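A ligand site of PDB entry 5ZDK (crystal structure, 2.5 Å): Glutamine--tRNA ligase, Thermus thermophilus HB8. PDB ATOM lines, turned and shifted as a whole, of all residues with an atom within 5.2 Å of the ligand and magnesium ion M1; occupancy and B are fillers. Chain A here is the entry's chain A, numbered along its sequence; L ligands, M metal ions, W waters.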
ATOM      1  N   PHE A  29      10.665 -24.744 -22.980  1.00  0.00           N
ATOM      2  CA  PHE A  29      10.625 -24.866 -21.492  1.00  0.00           C
ATOM      3  C   PHE A  29      11.806 -25.705 -20.951  1.00  0.00           C
ATOM      4  O   PHE A  29      11.961 -26.902 -21.334  1.00  0.00           O
ATOM      5  CB  PHE A  29       9.302 -25.440 -21.054  1.00  0.00           C
ATOM      6  CG  PHE A  29       9.212 -25.721 -19.572  1.00  0.00           C
ATOM      7  CD1 PHE A  29       9.305 -24.663 -18.630  1.00  0.00           C
ATOM      8  CD2 PHE A  29       8.962 -27.015 -19.108  1.00  0.00           C
ATOM      9  CE1 PHE A  29       9.171 -24.912 -17.286  1.00  0.00           C
ATOM     10  CE2 PHE A  29       8.824 -27.251 -17.746  1.00  0.00           C
ATOM     11  CZ  PHE A  29       8.915 -26.186 -16.847  1.00  0.00           C
ATOM     12  N   PRO A  30      12.655 -25.104 -20.090  1.00  0.00           N
ATOM     13  CA  PRO A  30      13.805 -25.933 -19.778  1.00  0.00           C
ATOM     14  C   PRO A  30      14.152 -26.547 -18.398  1.00  0.00           C
ATOM     15  O   PRO A  30      15.322 -26.616 -18.086  1.00  0.00           O
ATOM     16  CB  PRO A  30      14.989 -25.059 -20.260  1.00  0.00           C
ATOM     17  CG  PRO A  30      14.533 -23.642 -19.959  1.00  0.00           C
ATOM     18  CD  PRO A  30      12.988 -23.659 -19.920  1.00  0.00           C
ATOM     19  N   PRO A  31      13.206 -27.128 -17.673  1.00  0.00           N
ATOM     20  CA  PRO A  31      13.554 -27.395 -16.266  1.00  0.00           C
ATOM     21  C   PRO A  31      14.645 -28.429 -16.078  1.00  0.00           C
ATOM     22  O   PRO A  31      15.030 -29.160 -17.043  1.00  0.00           O
ATOM     23  CB  PRO A  31      12.266 -27.975 -15.719  1.00  0.00           C
ATOM     24  CG  PRO A  31      11.799 -28.855 -16.895  1.00  0.00           C
ATOM     25  CD  PRO A  31      12.171 -28.080 -18.155  1.00  0.00           C
ATOM     26  N   GLU A  32      15.099 -28.523 -14.823  1.00  0.00           N
ATOM     27  CA  GLU A  32      16.205 -29.391 -14.414  1.00  0.00           C
ATOM     28  C   GLU A  32      15.573 -30.708 -13.992  1.00  0.00           C
ATOM     29  O   GLU A  32      14.657 -30.711 -13.215  1.00  0.00           O
ATOM     30  CB  GLU A  32      16.971 -28.800 -13.221  1.00  0.00           C
ATOM     31  CG  GLU A  32      17.349 -27.326 -13.308  1.00  0.00           C
ATOM     32  CD  GLU A  32      18.266 -26.856 -12.154  1.00  0.00           C
ATOM     33  OE1 GLU A  32      17.796 -26.599 -11.003  1.00  0.00           O
ATOM     34  OE2 GLU A  32      19.468 -26.750 -12.385  1.00  0.00           O
ATOM     35  N   HIS A  38       6.071 -27.550  -9.842  1.00  0.00           N
ATOM     36  CA  HIS A  38       5.024 -26.964  -8.990  1.00  0.00           C
ATOM     37  C   HIS A  38       4.224 -25.852  -9.751  1.00  0.00           C
ATOM     38  O   HIS A  38       4.577 -25.506 -10.883  1.00  0.00           O
ATOM     39  CB  HIS A  38       5.625 -26.446  -7.645  1.00  0.00           C
ATOM     40  CG  HIS A  38       6.716 -25.404  -7.818  1.00  0.00           C
ATOM     41  ND1 HIS A  38       6.520 -24.212  -8.477  1.00  0.00           N
ATOM     42  CD2 HIS A  38       8.007 -25.392  -7.402  1.00  0.00           C
ATOM     43  CE1 HIS A  38       7.658 -23.516  -8.488  1.00  0.00           C
ATOM     44  NE2 HIS A  38       8.572 -24.216  -7.852  1.00  0.00           N
ATOM     45  N   GLY A  40       4.280 -22.532  -9.696  1.00  0.00           N
ATOM     46  CA  GLY A  40       5.194 -21.585 -10.306  1.00  0.00           C
ATOM     47  C   GLY A  40       5.678 -22.053 -11.681  1.00  0.00           C
ATOM     48  O   GLY A  40       5.556 -21.318 -12.674  1.00  0.00           O
ATOM     49  N   HIS A  41       6.247 -23.258 -11.790  1.00  0.00           N
ATOM     50  CA  HIS A  41       6.618 -23.730 -13.124  1.00  0.00           C
ATOM     51  C   HIS A  41       5.445 -23.645 -14.131  1.00  0.00           C
ATOM     52  O   HIS A  41       5.636 -23.311 -15.274  1.00  0.00           O
ATOM     53  CB  HIS A  41       7.182 -25.145 -13.089  1.00  0.00           C
ATOM     54  CG  HIS A  41       8.388 -25.292 -12.201  1.00  0.00           C
ATOM     55  ND1 HIS A  41       8.300 -25.789 -10.911  1.00  0.00           N
ATOM     56  CD2 HIS A  41       9.688 -24.996 -12.413  1.00  0.00           C
ATOM     57  CE1 HIS A  41       9.512 -25.809 -10.378  1.00  0.00           C
ATOM     58  NE2 HIS A  41      10.371 -25.317 -11.265  1.00  0.00           N
ATOM     59  N   ARG A  43       3.507 -21.280 -14.762  1.00  0.00           N
ATOM     60  CA  ARG A  43       3.582 -20.008 -15.536  1.00  0.00           C
ATOM     61  C   ARG A  43       4.548 -20.097 -16.768  1.00  0.00           C
ATOM     62  O   ARG A  43       4.177 -19.645 -17.877  1.00  0.00           O
ATOM     63  CB  ARG A  43       3.948 -18.815 -14.647  1.00  0.00           C
ATOM     64  CG  ARG A  43       4.217 -17.535 -15.406  1.00  0.00           C
ATOM     65  CD  ARG A  43       4.411 -16.371 -14.461  1.00  0.00           C
ATOM     66  NE  ARG A  43       3.169 -16.053 -13.755  1.00  0.00           N
ATOM     67  CZ  ARG A  43       3.013 -15.107 -12.823  1.00  0.00           C
ATOM     68  NH1 ARG A  43       4.048 -14.343 -12.382  1.00  0.00           N
ATOM     69  NH2 ARG A  43       1.787 -14.940 -12.308  1.00  0.00           N
ATOM     70  N   SER A  44       5.742 -20.663 -16.548  1.00  0.00           N
ATOM     71  CA  SER A  44       6.721 -20.869 -17.595  1.00  0.00           C
ATOM     72  C   SER A  44       6.225 -21.911 -18.678  1.00  0.00           C
ATOM     73  O   SER A  44       6.528 -21.788 -19.873  1.00  0.00           O
ATOM     74  CB  SER A  44       8.046 -21.329 -16.983  1.00  0.00           C
ATOM     75  OG  SER A  44       9.066 -21.342 -17.992  1.00  0.00           O
ATOM     76  N   LEU A 221      12.823 -17.534 -23.055  1.00  0.00           N
ATOM     77  CA  LEU A 221      12.111 -16.866 -21.954  1.00  0.00           C
ATOM     78  C   LEU A 221      12.426 -17.333 -20.529  1.00  0.00           C
ATOM     79  O   LEU A 221      12.133 -18.477 -20.121  1.00  0.00           O
ATOM     80  CB  LEU A 221      10.637 -16.941 -22.181  1.00  0.00           C
ATOM     81  CG  LEU A 221      10.230 -16.486 -23.565  1.00  0.00           C
ATOM     82  CD1 LEU A 221       8.735 -16.568 -23.689  1.00  0.00           C
ATOM     83  CD2 LEU A 221      10.685 -15.061 -23.798  1.00  0.00           C
ATOM     84  N   CYS A 222      12.987 -16.413 -19.752  1.00  0.00           N
ATOM     85  CA  CYS A 222      13.482 -16.719 -18.406  1.00  0.00           C
ATOM     86  C   CYS A 222      12.867 -15.792 -17.363  1.00  0.00           C
ATOM     87  O   CYS A 222      12.382 -14.712 -17.696  1.00  0.00           O
ATOM     88  CB  CYS A 222      15.026 -16.662 -18.385  1.00  0.00           C
ATOM     89  SG  CYS A 222      15.721 -15.015 -18.751  1.00  0.00           S
ATOM     90  N   THR A 223      12.843 -16.231 -16.112  1.00  0.00           N
ATOM     91  CA  THR A 223      12.380 -15.428 -15.004  1.00  0.00           C
ATOM     92  C   THR A 223      13.518 -14.523 -14.653  1.00  0.00           C
ATOM     93  O   THR A 223      14.650 -14.787 -15.089  1.00  0.00           O
ATOM     94  CB  THR A 223      12.129 -16.262 -13.755  1.00  0.00           C
ATOM     95  OG1 THR A 223      13.352 -16.907 -13.371  1.00  0.00           O
ATOM     96  CG2 THR A 223      11.084 -17.286 -13.999  1.00  0.00           C
ATOM     97  N   GLU A 225      15.604 -13.688 -12.332  1.00  0.00           N
ATOM     98  CA  GLU A 225      16.887 -13.948 -11.648  1.00  0.00           C
ATOM     99  C   GLU A 225      18.095 -13.759 -12.588  1.00  0.00           C
ATOM    100  O   GLU A 225      19.195 -13.425 -12.150  1.00  0.00           O
ATOM    101  CB  GLU A 225      16.917 -15.331 -10.957  1.00  0.00           C
ATOM    102  CG  GLU A 225      15.648 -15.735 -10.211  1.00  0.00           C
ATOM    103  CD  GLU A 225      15.003 -14.606  -9.385  1.00  0.00           C
ATOM    104  OE1 GLU A 225      15.653 -14.143  -8.405  1.00  0.00           O
ATOM    105  OE2 GLU A 225      13.850 -14.183  -9.719  1.00  0.00           O
ATOM    106  N   PHE A 257      10.313 -12.454 -17.514  1.00  0.00           N
ATOM    107  CA  PHE A 257       8.949 -12.271 -16.975  1.00  0.00           C
ATOM    108  C   PHE A 257       8.987 -12.506 -15.457  1.00  0.00           C
ATOM    109  O   PHE A 257       9.961 -13.070 -14.942  1.00  0.00           O
ATOM    110  CB  PHE A 257       7.919 -13.206 -17.705  1.00  0.00           C
ATOM    111  CG  PHE A 257       8.208 -14.680 -17.504  1.00  0.00           C
ATOM    112  CD1 PHE A 257       9.032 -15.363 -18.387  1.00  0.00           C
ATOM    113  CD2 PHE A 257       7.672 -15.363 -16.408  1.00  0.00           C
ATOM    114  CE1 PHE A 257       9.323 -16.698 -18.199  1.00  0.00           C
ATOM    115  CE2 PHE A 257       7.979 -16.695 -16.202  1.00  0.00           C
ATOM    116  CZ  PHE A 257       8.788 -17.368 -17.101  1.00  0.00           C
ATOM    117  N   ALA A 258       7.970 -12.076 -14.719  1.00  0.00           N
ATOM    118  CA  ALA A 258       8.045 -12.211 -13.262  1.00  0.00           C
ATOM    119  C   ALA A 258       7.672 -13.630 -12.842  1.00  0.00           C
ATOM    120  O   ALA A 258       6.697 -14.217 -13.344  1.00  0.00           O
ATOM    121  CB  ALA A 258       7.184 -11.190 -12.538  1.00  0.00           C
ATOM    122  N   ARG A 259       8.437 -14.162 -11.902  1.00  0.00           N
ATOM    123  CA  ARG A 259       8.260 -15.513 -11.434  1.00  0.00           C
ATOM    124  C   ARG A 259       7.082 -15.418 -10.533  1.00  0.00           C
ATOM    125  O   ARG A 259       6.868 -14.382  -9.958  1.00  0.00           O
ATOM    126  CB  ARG A 259       9.499 -16.022 -10.691  1.00  0.00           C
ATOM    127  CG  ARG A 259       9.863 -15.367  -9.352  1.00  0.00           C
ATOM    128  CD  ARG A 259      10.848 -16.247  -8.568  1.00  0.00           C
ATOM    129  NE  ARG A 259      11.948 -16.633  -9.445  1.00  0.00           N
ATOM    130  CZ  ARG A 259      12.421 -17.876  -9.584  1.00  0.00           C
ATOM    131  NH1 ARG A 259      11.916 -18.854  -8.875  1.00  0.00           N
ATOM    132  NH2 ARG A 259      13.411 -18.136 -10.425  1.00  0.00           N
ATOM    133  N   LEU A 260       6.320 -16.488 -10.416  1.00  0.00           N
ATOM    134  CA  LEU A 260       5.147 -16.490  -9.588  1.00  0.00           C
ATOM    135  C   LEU A 260       5.525 -16.747  -8.121  1.00  0.00           C
ATOM    136  O   LEU A 260       6.393 -17.587  -7.804  1.00  0.00           O
ATOM    137  CB  LEU A 260       4.105 -17.499 -10.117  1.00  0.00           C
ATOM    138  CG  LEU A 260       3.015 -17.987  -9.164  1.00  0.00           C
ATOM    139  CD1 LEU A 260       2.083 -16.863  -8.737  1.00  0.00           C
ATOM    140  CD2 LEU A 260       2.238 -19.219  -9.659  1.00  0.00           C
ATOM    141  N   ASP A 261       4.891 -15.964  -7.249  1.00  0.00           N
ATOM    142  CA  ASP A 261       5.060 -16.085  -5.797  1.00  0.00           C
ATOM    143  C   ASP A 261       3.638 -15.959  -5.363  1.00  0.00           C
ATOM    144  O   ASP A 261       2.949 -14.958  -5.668  1.00  0.00           O
ATOM    145  CB  ASP A 261       5.941 -14.945  -5.230  1.00  0.00           C
ATOM    146  CG  ASP A 261       5.655 -14.568  -3.716  1.00  0.00           C
ATOM    147  OD1 ASP A 261       5.106 -15.344  -2.843  1.00  0.00           O
ATOM    148  OD2 ASP A 261       6.047 -13.403  -3.397  1.00  0.00           O
ATOM    149  N   LEU A 267       7.493 -22.396  -2.650  1.00  0.00           N
ATOM    150  CA  LEU A 267       7.877 -23.105  -3.851  1.00  0.00           C
ATOM    151  C   LEU A 267       9.373 -23.474  -3.924  1.00  0.00           C
ATOM    152  O   LEU A 267       9.793 -24.102  -4.925  1.00  0.00           O
ATOM    153  CB  LEU A 267       7.519 -22.257  -5.065  1.00  0.00           C
ATOM    154  CG  LEU A 267       6.051 -21.822  -5.206  1.00  0.00           C
ATOM    155  CD1 LEU A 267       5.862 -20.946  -6.423  1.00  0.00           C
ATOM    156  CD2 LEU A 267       5.129 -23.021  -5.274  1.00  0.00           C
ATOM    157  N   LYS A 269      12.806 -25.358  -3.608  1.00  0.00           N
ATOM    158  CA  LYS A 269      13.099 -26.792  -3.566  1.00  0.00           C
ATOM    159  C   LYS A 269      13.584 -27.169  -2.178  1.00  0.00           C
ATOM    160  O   LYS A 269      13.154 -28.187  -1.622  1.00  0.00           O
ATOM    161  CB  LYS A 269      14.152 -27.197  -4.620  1.00  0.00           C
ATOM    162  CG  LYS A 269      14.098 -28.683  -4.962  1.00  0.00           C
ATOM    163  CD  LYS A 269      15.433 -29.273  -5.409  1.00  0.00           C
ATOM    164  CE  LYS A 269      15.760 -29.001  -6.876  1.00  0.00           C
ATOM    165  NZ  LYS A 269      17.170 -29.380  -7.248  1.00  0.00           N
HETATM  166  P1  LIG L   1      15.175 -21.226 -10.800  1.00  0.00           P
HETATM  167  O1  LIG L   1      16.582 -21.514 -10.281  1.00  0.00           O
HETATM  168  O2  LIG L   1      14.054 -21.712  -9.943  1.00  0.00           O
HETATM  169  O3  LIG L   1      14.903 -19.857 -11.357  1.00  0.00           O
HETATM  170  P2  LIG L   1      15.753 -23.718 -11.926  1.00  0.00           P
HETATM  171  O4  LIG L   1      17.187 -23.764 -12.461  1.00  0.00           O
HETATM  172  O5  LIG L   1      15.340 -24.162 -10.508  1.00  0.00           O
HETATM  173  O6  LIG L   1      15.198 -22.208 -12.074  1.00  0.00           O
HETATM  174  P3  LIG L   1      13.531 -25.285 -12.751  1.00  0.00           P
HETATM  175  O7  LIG L   1      14.051 -26.571 -13.326  1.00  0.00           O
HETATM  176  O8  LIG L   1      13.213 -25.091 -11.282  1.00  0.00           O
HETATM  177  O9  LIG L   1      14.823 -24.397 -13.061  1.00  0.00           O
HETATM  178  O10 LIG L   1      12.467 -24.444 -13.645  1.00  0.00           O
HETATM  179  C1  LIG L   1      12.557 -24.336 -15.076  1.00  0.00           C
HETATM  180  C2  LIG L   1      12.074 -22.982 -15.600  1.00  0.00           C
HETATM  181  O11 LIG L   1      10.863 -22.580 -14.940  1.00  0.00           O
HETATM  182  C3  LIG L   1      13.064 -21.901 -15.274  1.00  0.00           C
HETATM  183  O12 LIG L   1      12.977 -20.956 -16.345  1.00  0.00           O
HETATM  184  C4  LIG L   1      12.561 -21.339 -13.935  1.00  0.00           C
HETATM  185  O13 LIG L   1      13.067 -20.039 -13.538  1.00  0.00           O
HETATM  186  C5  LIG L   1      11.068 -21.365 -14.193  1.00  0.00           C
HETATM  187  N1  LIG L   1      10.393 -21.229 -12.878  1.00  0.00           N
HETATM  188  C6  LIG L   1      10.735 -21.831 -11.712  1.00  0.00           C
HETATM  189  N2  LIG L   1       9.945 -21.380 -10.695  1.00  0.00           N
HETATM  190  C7  LIG L   1       9.087 -20.494 -11.217  1.00  0.00           C
HETATM  191  C8  LIG L   1       7.999 -19.654 -10.718  1.00  0.00           C
HETATM  192  N3  LIG L   1       7.686 -19.718  -9.397  1.00  0.00           N
HETATM  193  N4  LIG L   1       7.342 -18.834 -11.587  1.00  0.00           N
HETATM  194  C9  LIG L   1       7.673 -18.761 -12.882  1.00  0.00           C
HETATM  195  N5  LIG L   1       8.673 -19.515 -13.374  1.00  0.00           N
HETATM  196  C10 LIG L   1       9.393 -20.372 -12.631  1.00  0.00           C
HETATM  197 MG    MG M   1      14.013 -25.661  -9.253  1.00  0.00          MG
HETATM  198 MG    MG M   2      18.111 -23.600  -9.093  1.00  0.00          MG
HETATM  199  O   HOH W   1      10.948 -22.607  -7.888  1.00  0.00           O
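Magnesium ion M1 is bound by O8 of the ligand, at 2.3 Å.
Magnesium ion M1 is bound by an oxygen (O5) of the ligand (2.4 Å).
N of Leu 260 sits at hydrogen-bond distance from N4 of the ligand (2.8 Å).
O of Leu 260 sits at hydrogen-bond distance from N3 of the ligand (3.0 Å).
An oxygen (O3) of the ligand is in salt-bridge range of the guanidinium group (NH2) of Arg 259 (2.5 Å).
An oxygen (O10) of the ligand lies close to a ring nitrogen (NE2) of His 41 (3.3 Å).
The side-chain hydroxyl (OG1) of Thr 223 lies within hydrogen-bond range of an oxygen (O13) of the ligand (3.1 Å).
The backbone NH (N) of Glu 32 is in hydrogen-bond range of an oxygen (O7) of the ligand (2.7 Å).
No residue comes within 4 Å of magnesium ion M1.
The nearest printed residue that does not touch magnesium ion M1 is His 41 (4.2 Å).
The backbone NH of Gly 40 sits at hydrogen-bond distance from a ring nitrogen (ND1) of His 38 (3.1 Å).
The side-chain carboxylate (OE2) of Glu 225 is in salt-bridge range of the guanidinium group (NE) of Arg 259, at 3.1 Å.
The backbone carbonyl oxygen (O) of Cys 222 is in hydrogen-bond range of the backbone NH (N) of Phe 257, at 3.1 Å.
NE2 of His 38 is in hydrogen-bond range of O of Leu 267 (3.2 Å).
A ring nitrogen (ND1) of His 41 lies within hydrogen-bond range of the backbone NH (N) of His 38 (3.0 Å).
NH2 of Arg 259 is in hydrogen-bond range of OG1 of Thr 223 (3.2 Å).
N4 of the ligand lies close to O of Gly 40 (3.2 Å).
Merely in contact with the ligand: Phe 29, Pro 31, His 38, Ser 44, Phe 257 and Leu 267.
Of the 20 residues printed, 12 come within 4 Å of the ligand.
The nearest printed residue that does not touch the ligand is Arg 43 (4.1 Å).
Water W1 lies within hydrogen-bond range of NE2 of His 38 (2.9 Å) and N2 of the ligand (3.2 Å).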
